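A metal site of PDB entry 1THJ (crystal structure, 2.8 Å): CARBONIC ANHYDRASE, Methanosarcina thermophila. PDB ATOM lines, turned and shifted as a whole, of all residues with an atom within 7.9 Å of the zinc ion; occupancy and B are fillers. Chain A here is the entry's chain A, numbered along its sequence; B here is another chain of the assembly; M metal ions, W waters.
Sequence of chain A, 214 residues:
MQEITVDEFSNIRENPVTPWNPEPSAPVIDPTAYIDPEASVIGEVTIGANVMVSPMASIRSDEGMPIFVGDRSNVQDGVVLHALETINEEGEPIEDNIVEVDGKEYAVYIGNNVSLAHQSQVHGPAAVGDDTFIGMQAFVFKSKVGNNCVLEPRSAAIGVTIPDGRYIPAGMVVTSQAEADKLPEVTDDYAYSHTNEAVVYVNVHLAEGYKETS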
ATOM      1  N   ARG A  60     -24.326   4.107  13.047  1.00  0.00           N
ATOM      2  CA  ARG A  60     -24.890   4.911  14.129  1.00  0.00           C
ATOM      3  C   ARG A  60     -23.883   5.646  14.988  1.00  0.00           C
ATOM      4  O   ARG A  60     -23.350   5.130  15.976  1.00  0.00           O
ATOM      5  CB  ARG A  60     -25.761   3.988  14.982  1.00  0.00           C
ATOM      6  CG  ARG A  60     -26.546   4.618  16.109  1.00  0.00           C
ATOM      7  CD  ARG A  60     -27.368   3.530  16.828  1.00  0.00           C
ATOM      8  NE  ARG A  60     -27.093   3.527  18.259  1.00  0.00           N
ATOM      9  CZ  ARG A  60     -27.106   2.436  19.006  1.00  0.00           C
ATOM     10  NH1 ARG A  60     -27.362   1.280  18.448  1.00  0.00           N
ATOM     11  NH2 ARG A  60     -26.820   2.492  20.298  1.00  0.00           N
ATOM     12  N   ASP A  62     -23.813   8.021  17.509  1.00  0.00           N
ATOM     13  CA  ASP A  62     -24.506   8.759  18.566  1.00  0.00           C
ATOM     14  C   ASP A  62     -23.821   8.699  19.910  1.00  0.00           C
ATOM     15  O   ASP A  62     -24.138   9.474  20.800  1.00  0.00           O
ATOM     16  CB  ASP A  62     -25.942   8.276  18.686  1.00  0.00           C
ATOM     17  CG  ASP A  62     -26.032   6.783  18.917  1.00  0.00           C
ATOM     18  OD1 ASP A  62     -25.023   6.074  18.765  1.00  0.00           O
ATOM     19  OD2 ASP A  62     -27.134   6.303  19.249  1.00  0.00           O
ATOM     20  N   GLU A  63     -22.947   7.727  20.081  1.00  0.00           N
ATOM     21  CA  GLU A  63     -22.206   7.606  21.339  1.00  0.00           C
ATOM     22  C   GLU A  63     -20.820   8.201  21.060  1.00  0.00           C
ATOM     23  O   GLU A  63     -20.497   9.313  21.494  1.00  0.00           O
ATOM     24  CB  GLU A  63     -22.081   6.132  21.771  1.00  0.00           C
ATOM     25  CG  GLU A  63     -21.485   5.943  23.180  1.00  0.00           C
ATOM     26  CD  GLU A  63     -21.218   4.487  23.593  1.00  0.00           C
ATOM     27  OE1 GLU A  63     -21.929   3.553  23.144  1.00  0.00           O
ATOM     28  OE2 GLU A  63     -20.289   4.290  24.391  1.00  0.00           O
ATOM     29  N   GLY A  64     -20.020   7.462  20.289  1.00  0.00           N
ATOM     30  CA  GLY A  64     -18.695   7.932  19.941  1.00  0.00           C
ATOM     31  C   GLY A  64     -18.808   8.445  18.536  1.00  0.00           C
ATOM     32  O   GLY A  64     -19.355   7.761  17.666  1.00  0.00           O
ATOM     33  N   VAL A  80     -22.743  -3.223  10.853  1.00  0.00           N
ATOM     34  CA  VAL A  80     -23.043  -2.274  11.914  1.00  0.00           C
ATOM     35  C   VAL A  80     -21.812  -1.494  12.256  1.00  0.00           C
ATOM     36  O   VAL A  80     -20.734  -2.076  12.357  1.00  0.00           O
ATOM     37  CB  VAL A  80     -23.456  -2.987  13.219  1.00  0.00           C
ATOM     38  CG1 VAL A  80     -23.583  -1.998  14.358  1.00  0.00           C
ATOM     39  CG2 VAL A  80     -24.743  -3.702  13.020  1.00  0.00           C
ATOM     40  N   LEU A  81     -21.970  -0.202  12.448  1.00  0.00           N
ATOM     41  CA  LEU A  81     -20.838   0.623  12.820  1.00  0.00           C
ATOM     42  C   LEU A  81     -21.298   1.332  14.039  1.00  0.00           C
ATOM     43  O   LEU A  81     -22.450   1.737  14.107  1.00  0.00           O
ATOM     44  CB  LEU A  81     -20.528   1.634  11.758  1.00  0.00           C
ATOM     45  CG  LEU A  81     -20.258   1.057  10.376  1.00  0.00           C
ATOM     46  CD1 LEU A  81     -19.435   2.082   9.649  1.00  0.00           C
ATOM     47  CD2 LEU A  81     -19.497  -0.217  10.435  1.00  0.00           C
ATOM     48  N   HIS A  82     -20.430   1.451  15.031  1.00  0.00           N
ATOM     49  CA  HIS A  82     -20.771   2.144  16.261  1.00  0.00           C
ATOM     50  C   HIS A  82     -19.455   2.380  16.989  1.00  0.00           C
ATOM     51  O   HIS A  82     -18.472   1.755  16.652  1.00  0.00           O
ATOM     52  CB  HIS A  82     -21.710   1.297  17.093  1.00  0.00           C
ATOM     53  CG  HIS A  82     -22.391   2.065  18.183  1.00  0.00           C
ATOM     54  ND1 HIS A  82     -22.313   1.676  19.499  1.00  0.00           N
ATOM     55  CD2 HIS A  82     -23.109   3.204  18.093  1.00  0.00           C
ATOM     56  CE1 HIS A  82     -22.978   2.584  20.181  1.00  0.00           C
ATOM     57  NE2 HIS A  82     -23.486   3.539  19.365  1.00  0.00           N
ATOM     58  N   ALA A  83     -19.418   3.239  17.999  1.00  0.00           N
ATOM     59  CA  ALA A  83     -18.165   3.517  18.694  1.00  0.00           C
ATOM     60  C   ALA A  83     -18.395   3.824  20.156  1.00  0.00           C
ATOM     61  O   ALA A  83     -19.534   4.047  20.572  1.00  0.00           O
ATOM     62  CB  ALA A  83     -17.473   4.681  18.053  1.00  0.00           C
ATOM     63  N   LEU A  84     -17.332   3.811  20.935  1.00  0.00           N
ATOM     64  CA  LEU A  84     -17.462   4.072  22.366  1.00  0.00           C
ATOM     65  C   LEU A  84     -17.369   5.560  22.610  1.00  0.00           C
ATOM     66  O   LEU A  84     -16.660   6.261  21.878  1.00  0.00           O
ATOM     67  CB  LEU A  84     -16.386   3.327  23.133  1.00  0.00           C
ATOM     68  CG  LEU A  84     -16.524   1.805  23.118  1.00  0.00           C
ATOM     69  CD1 LEU A  84     -15.164   1.158  23.045  1.00  0.00           C
ATOM     70  CD2 LEU A  84     -17.262   1.344  24.348  1.00  0.00           C
ATOM     71  N   GLU A  85     -18.081   6.042  23.623  1.00  0.00           N
ATOM     72  CA  GLU A  85     -18.122   7.464  23.969  1.00  0.00           C
ATOM     73  C   GLU A  85     -16.780   8.169  23.788  1.00  0.00           C
ATOM     74  O   GLU A  85     -15.816   7.885  24.487  1.00  0.00           O
ATOM     75  CB  GLU A  85     -18.627   7.635  25.408  1.00  0.00           C
ATOM     76  CG  GLU A  85     -19.122   9.034  25.748  1.00  0.00           C
ATOM     77  CD  GLU A  85     -19.652   9.157  27.162  1.00  0.00           C
ATOM     78  OE1 GLU A  85     -20.002   8.120  27.764  1.00  0.00           O
ATOM     79  OE2 GLU A  85     -19.721  10.281  27.688  1.00  0.00           O
ATOM     80  N   GLN A 121     -18.907  -6.258  11.334  1.00  0.00           N
ATOM     81  CA  GLN A 121     -19.232  -5.180  12.271  1.00  0.00           C
ATOM     82  C   GLN A 121     -17.922  -4.542  12.591  1.00  0.00           C
ATOM     83  O   GLN A 121     -16.918  -5.230  12.692  1.00  0.00           O
ATOM     84  CB  GLN A 121     -19.870  -5.698  13.578  1.00  0.00           C
ATOM     85  CG  GLN A 121     -19.872  -4.638  14.678  1.00  0.00           C
ATOM     86  CD  GLN A 121     -20.530  -5.049  15.991  1.00  0.00           C
ATOM     87  OE1 GLN A 121     -20.546  -4.272  16.971  1.00  0.00           O
ATOM     88  NE2 GLN A 121     -21.089  -6.237  16.026  1.00  0.00           N
ATOM     89  N   VAL A 122     -17.910  -3.238  12.763  1.00  0.00           N
ATOM     90  CA  VAL A 122     -16.689  -2.538  13.105  1.00  0.00           C
ATOM     91  C   VAL A 122     -17.106  -1.592  14.192  1.00  0.00           C
ATOM     92  O   VAL A 122     -18.042  -0.803  13.999  1.00  0.00           O
ATOM     93  CB  VAL A 122     -16.142  -1.753  11.930  1.00  0.00           C
ATOM     94  CG1 VAL A 122     -14.901  -0.948  12.363  1.00  0.00           C
ATOM     95  CG2 VAL A 122     -15.804  -2.705  10.792  1.00  0.00           C
ATOM     96  N   HIS A 123     -16.422  -1.658  15.316  1.00  0.00           N
ATOM     97  CA  HIS A 123     -16.769  -0.847  16.458  1.00  0.00           C
ATOM     98  C   HIS A 123     -15.613   0.013  16.963  1.00  0.00           C
ATOM     99  O   HIS A 123     -14.520  -0.448  17.190  1.00  0.00           O
ATOM    100  CB  HIS A 123     -17.272  -1.771  17.559  1.00  0.00           C
ATOM    101  CG  HIS A 123     -18.059  -1.063  18.617  1.00  0.00           C
ATOM    102  ND1 HIS A 123     -17.518  -0.141  19.482  1.00  0.00           N
ATOM    103  CD2 HIS A 123     -19.389  -1.106  18.887  1.00  0.00           C
ATOM    104  CE1 HIS A 123     -18.524   0.345  20.234  1.00  0.00           C
ATOM    105  NE2 HIS A 123     -19.691  -0.201  19.916  1.00  0.00           N
ATOM    106  N   GLY A 124     -15.876   1.289  17.168  1.00  0.00           N
ATOM    107  CA  GLY A 124     -14.834   2.180  17.605  1.00  0.00           C
ATOM    108  C   GLY A 124     -14.394   1.901  18.997  1.00  0.00           C
ATOM    109  O   GLY A 124     -15.177   1.365  19.793  1.00  0.00           O
ATOM    110  N   PHE A 141     -12.709  -4.503  16.582  1.00  0.00           N
ATOM    111  CA  PHE A 141     -13.041  -3.654  17.728  1.00  0.00           C
ATOM    112  C   PHE A 141     -11.755  -3.230  18.413  1.00  0.00           C
ATOM    113  O   PHE A 141     -10.832  -4.052  18.544  1.00  0.00           O
ATOM    114  CB  PHE A 141     -13.889  -4.490  18.696  1.00  0.00           C
ATOM    115  CG  PHE A 141     -14.161  -3.836  20.022  1.00  0.00           C
ATOM    116  CD1 PHE A 141     -14.346  -2.451  20.128  1.00  0.00           C
ATOM    117  CD2 PHE A 141     -14.327  -4.606  21.159  1.00  0.00           C
ATOM    118  CE1 PHE A 141     -14.678  -1.853  21.351  1.00  0.00           C
ATOM    119  CE2 PHE A 141     -14.662  -4.016  22.397  1.00  0.00           C
ATOM    120  CZ  PHE A 141     -14.851  -2.622  22.481  1.00  0.00           C
ATOM    121  N   GLN B  76     -29.377  -3.776  21.308  1.00  0.00           N
ATOM    122  CA  GLN B  76     -28.660  -3.018  20.274  1.00  0.00           C
ATOM    123  C   GLN B  76     -28.926  -3.467  18.858  1.00  0.00           C
ATOM    124  O   GLN B  76     -29.626  -4.448  18.641  1.00  0.00           O
ATOM    125  CB  GLN B  76     -27.169  -3.008  20.576  1.00  0.00           C
ATOM    126  CG  GLN B  76     -26.909  -2.648  22.014  1.00  0.00           C
ATOM    127  CD  GLN B  76     -25.479  -2.357  22.314  1.00  0.00           C
ATOM    128  OE1 GLN B  76     -24.613  -2.381  21.423  1.00  0.00           O
ATOM    129  NE2 GLN B  76     -25.185  -2.040  23.563  1.00  0.00           N
ATOM    130  N   ASP B  77     -28.330  -2.758  17.904  1.00  0.00           N
ATOM    131  CA  ASP B  77     -28.549  -3.024  16.481  1.00  0.00           C
ATOM    132  C   ASP B  77     -28.354  -4.471  16.125  1.00  0.00           C
ATOM    133  O   ASP B  77     -27.428  -5.092  16.596  1.00  0.00           O
ATOM    134  CB  ASP B  77     -27.619  -2.197  15.615  1.00  0.00           C
ATOM    135  CG  ASP B  77     -27.250  -0.876  16.239  1.00  0.00           C
ATOM    136  OD1 ASP B  77     -26.762  -0.876  17.390  1.00  0.00           O
ATOM    137  OD2 ASP B  77     -27.396   0.161  15.536  1.00  0.00           O
ATOM    138  N   ALA B 117     -25.403  -6.441  23.274  1.00  0.00           N
ATOM    139  CA  ALA B 117     -24.680  -5.649  22.294  1.00  0.00           C
ATOM    140  C   ALA B 117     -24.875  -6.016  20.823  1.00  0.00           C
ATOM    141  O   ALA B 117     -25.374  -7.092  20.475  1.00  0.00           O
ATOM    142  CB  ALA B 117     -23.218  -5.628  22.652  1.00  0.00           C
ATOM    143  N   HIS B 118     -24.473  -5.081  19.968  1.00  0.00           N
ATOM    144  CA  HIS B 118     -24.606  -5.190  18.555  1.00  0.00           C
ATOM    145  C   HIS B 118     -24.424  -6.584  18.053  1.00  0.00           C
ATOM    146  O   HIS B 118     -23.443  -7.224  18.306  1.00  0.00           O
ATOM    147  CB  HIS B 118     -23.565  -4.355  17.861  1.00  0.00           C
ATOM    148  CG  HIS B 118     -23.439  -2.965  18.404  1.00  0.00           C
ATOM    149  ND1 HIS B 118     -24.207  -1.910  18.008  1.00  0.00           N
ATOM    150  CD2 HIS B 118     -22.545  -2.449  19.287  1.00  0.00           C
ATOM    151  CE1 HIS B 118     -23.759  -0.820  18.652  1.00  0.00           C
ATOM    152  NE2 HIS B 118     -22.731  -1.090  19.458  1.00  0.00           N
ATOM    153  N   PHE B 133     -23.278  -8.449  30.610  1.00  0.00           N
ATOM    154  CA  PHE B 133     -23.000  -7.817  29.337  1.00  0.00           C
ATOM    155  C   PHE B 133     -22.850  -8.855  28.281  1.00  0.00           C
ATOM    156  O   PHE B 133     -21.896  -9.591  28.286  1.00  0.00           O
ATOM    157  CB  PHE B 133     -21.722  -6.993  29.450  1.00  0.00           C
ATOM    158  CG  PHE B 133     -21.222  -6.443  28.152  1.00  0.00           C
ATOM    159  CD1 PHE B 133     -21.702  -5.244  27.657  1.00  0.00           C
ATOM    160  CD2 PHE B 133     -20.248  -7.105  27.434  1.00  0.00           C
ATOM    161  CE1 PHE B 133     -21.201  -4.707  26.466  1.00  0.00           C
ATOM    162  CE2 PHE B 133     -19.741  -6.569  26.237  1.00  0.00           C
ATOM    163  CZ  PHE B 133     -20.223  -5.378  25.771  1.00  0.00           C
ATOM    164  N   MET B 136     -20.730  -8.010  21.702  1.00  0.00           N
ATOM    165  CA  MET B 136     -20.982  -8.001  20.278  1.00  0.00           C
ATOM    166  C   MET B 136     -20.855  -9.370  19.666  1.00  0.00           C
ATOM    167  O   MET B 136     -19.927 -10.109  19.955  1.00  0.00           O
ATOM    168  CB  MET B 136     -20.073  -7.016  19.548  1.00  0.00           C
ATOM    169  CG  MET B 136     -20.105  -5.592  20.079  1.00  0.00           C
ATOM    170  SD  MET B 136     -18.963  -5.457  21.408  1.00  0.00           S
ATOM    171  CE  MET B 136     -19.364  -3.909  22.078  1.00  0.00           C
ATOM    172  N   VAL B 199     -22.127   1.153  29.215  1.00  0.00           N
ATOM    173  CA  VAL B 199     -23.064   0.899  28.133  1.00  0.00           C
ATOM    174  C   VAL B 199     -24.479   1.229  28.614  1.00  0.00           C
ATOM    175  O   VAL B 199     -25.193   1.996  27.965  1.00  0.00           O
ATOM    176  CB  VAL B 199     -22.913  -0.541  27.613  1.00  0.00           C
ATOM    177  CG1 VAL B 199     -24.122  -0.988  26.854  1.00  0.00           C
ATOM    178  CG2 VAL B 199     -21.708  -0.611  26.703  1.00  0.00           C
ATOM    179  N   VAL B 202     -25.033   5.047  28.844  1.00  0.00           N
ATOM    180  CA  VAL B 202     -25.189   5.608  27.526  1.00  0.00           C
ATOM    181  C   VAL B 202     -26.535   5.289  26.953  1.00  0.00           C
ATOM    182  O   VAL B 202     -27.282   6.188  26.598  1.00  0.00           O
ATOM    183  CB  VAL B 202     -24.131   5.067  26.609  1.00  0.00           C
ATOM    184  CG1 VAL B 202     -24.458   5.391  25.187  1.00  0.00           C
ATOM    185  CG2 VAL B 202     -22.801   5.672  26.975  1.00  0.00           C
ATOM    186  N   ASN B 203     -26.886   4.020  26.935  1.00  0.00           N
ATOM    187  CA  ASN B 203     -28.163   3.623  26.370  1.00  0.00           C
ATOM    188  C   ASN B 203     -29.394   4.195  27.040  1.00  0.00           C
ATOM    189  O   ASN B 203     -30.341   4.591  26.381  1.00  0.00           O
ATOM    190  CB  ASN B 203     -28.258   2.115  26.248  1.00  0.00           C
ATOM    191  CG  ASN B 203     -27.480   1.605  25.061  1.00  0.00           C
ATOM    192  OD1 ASN B 203     -28.040   1.420  23.966  1.00  0.00           O
ATOM    193  ND2 ASN B 203     -26.178   1.462  25.230  1.00  0.00           N
HETATM  194 ZN    ZN M   1     -21.538   0.187  20.697  1.00  0.00          ZN
HETATM  195  O   HOH W   1     -22.119  -0.738  22.364  1.00  0.00           O
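Water W1 binds the zinc ion (2.0 Å). A ring nitrogen (NE2) of His 123 binds the zinc ion (2.0 Å). The zinc ion is bound by a ring nitrogen (ND1) of His 82, 2.1 Å away. A ring nitrogen (NE2) of His 118 of chain B is bound to the zinc ion (2.1 Å). The zinc ion has four donor atoms within binding distance.
The backbone carbonyl oxygen of His 82 sits at hydrogen-bond distance from the backbone NH of Gly 124, at 2.7 Å. A ring nitrogen (NE2) of His 82 sits at hydrogen-bond distance from the side-chain carboxylate of Asp 62. The backbone carbonyl oxygen (O) of Val 122 is in hydrogen-bond range of the backbone NH (N) of His 82 (3.4 Å). N of His 118 of chain B lies close to OE1 of Gln 76 of chain B (3.1 Å). The backbone carbonyl oxygen of His 118 of chain B is in hydrogen-bond range of the side-chain amide nitrogen of Gln 121 (3.4 Å). The side-chain carboxylate (OD1) of Asp 77 of chain B is in hydrogen-bond range of a ring nitrogen (ND1) of His 118 of chain B, 2.8 Å away.
Of the 24 residues printed, 3 come within 4 Å of the zinc ion. The nearest printed residue that does not touch the zinc ion is Gln 76 of chain B (4.1 Å).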
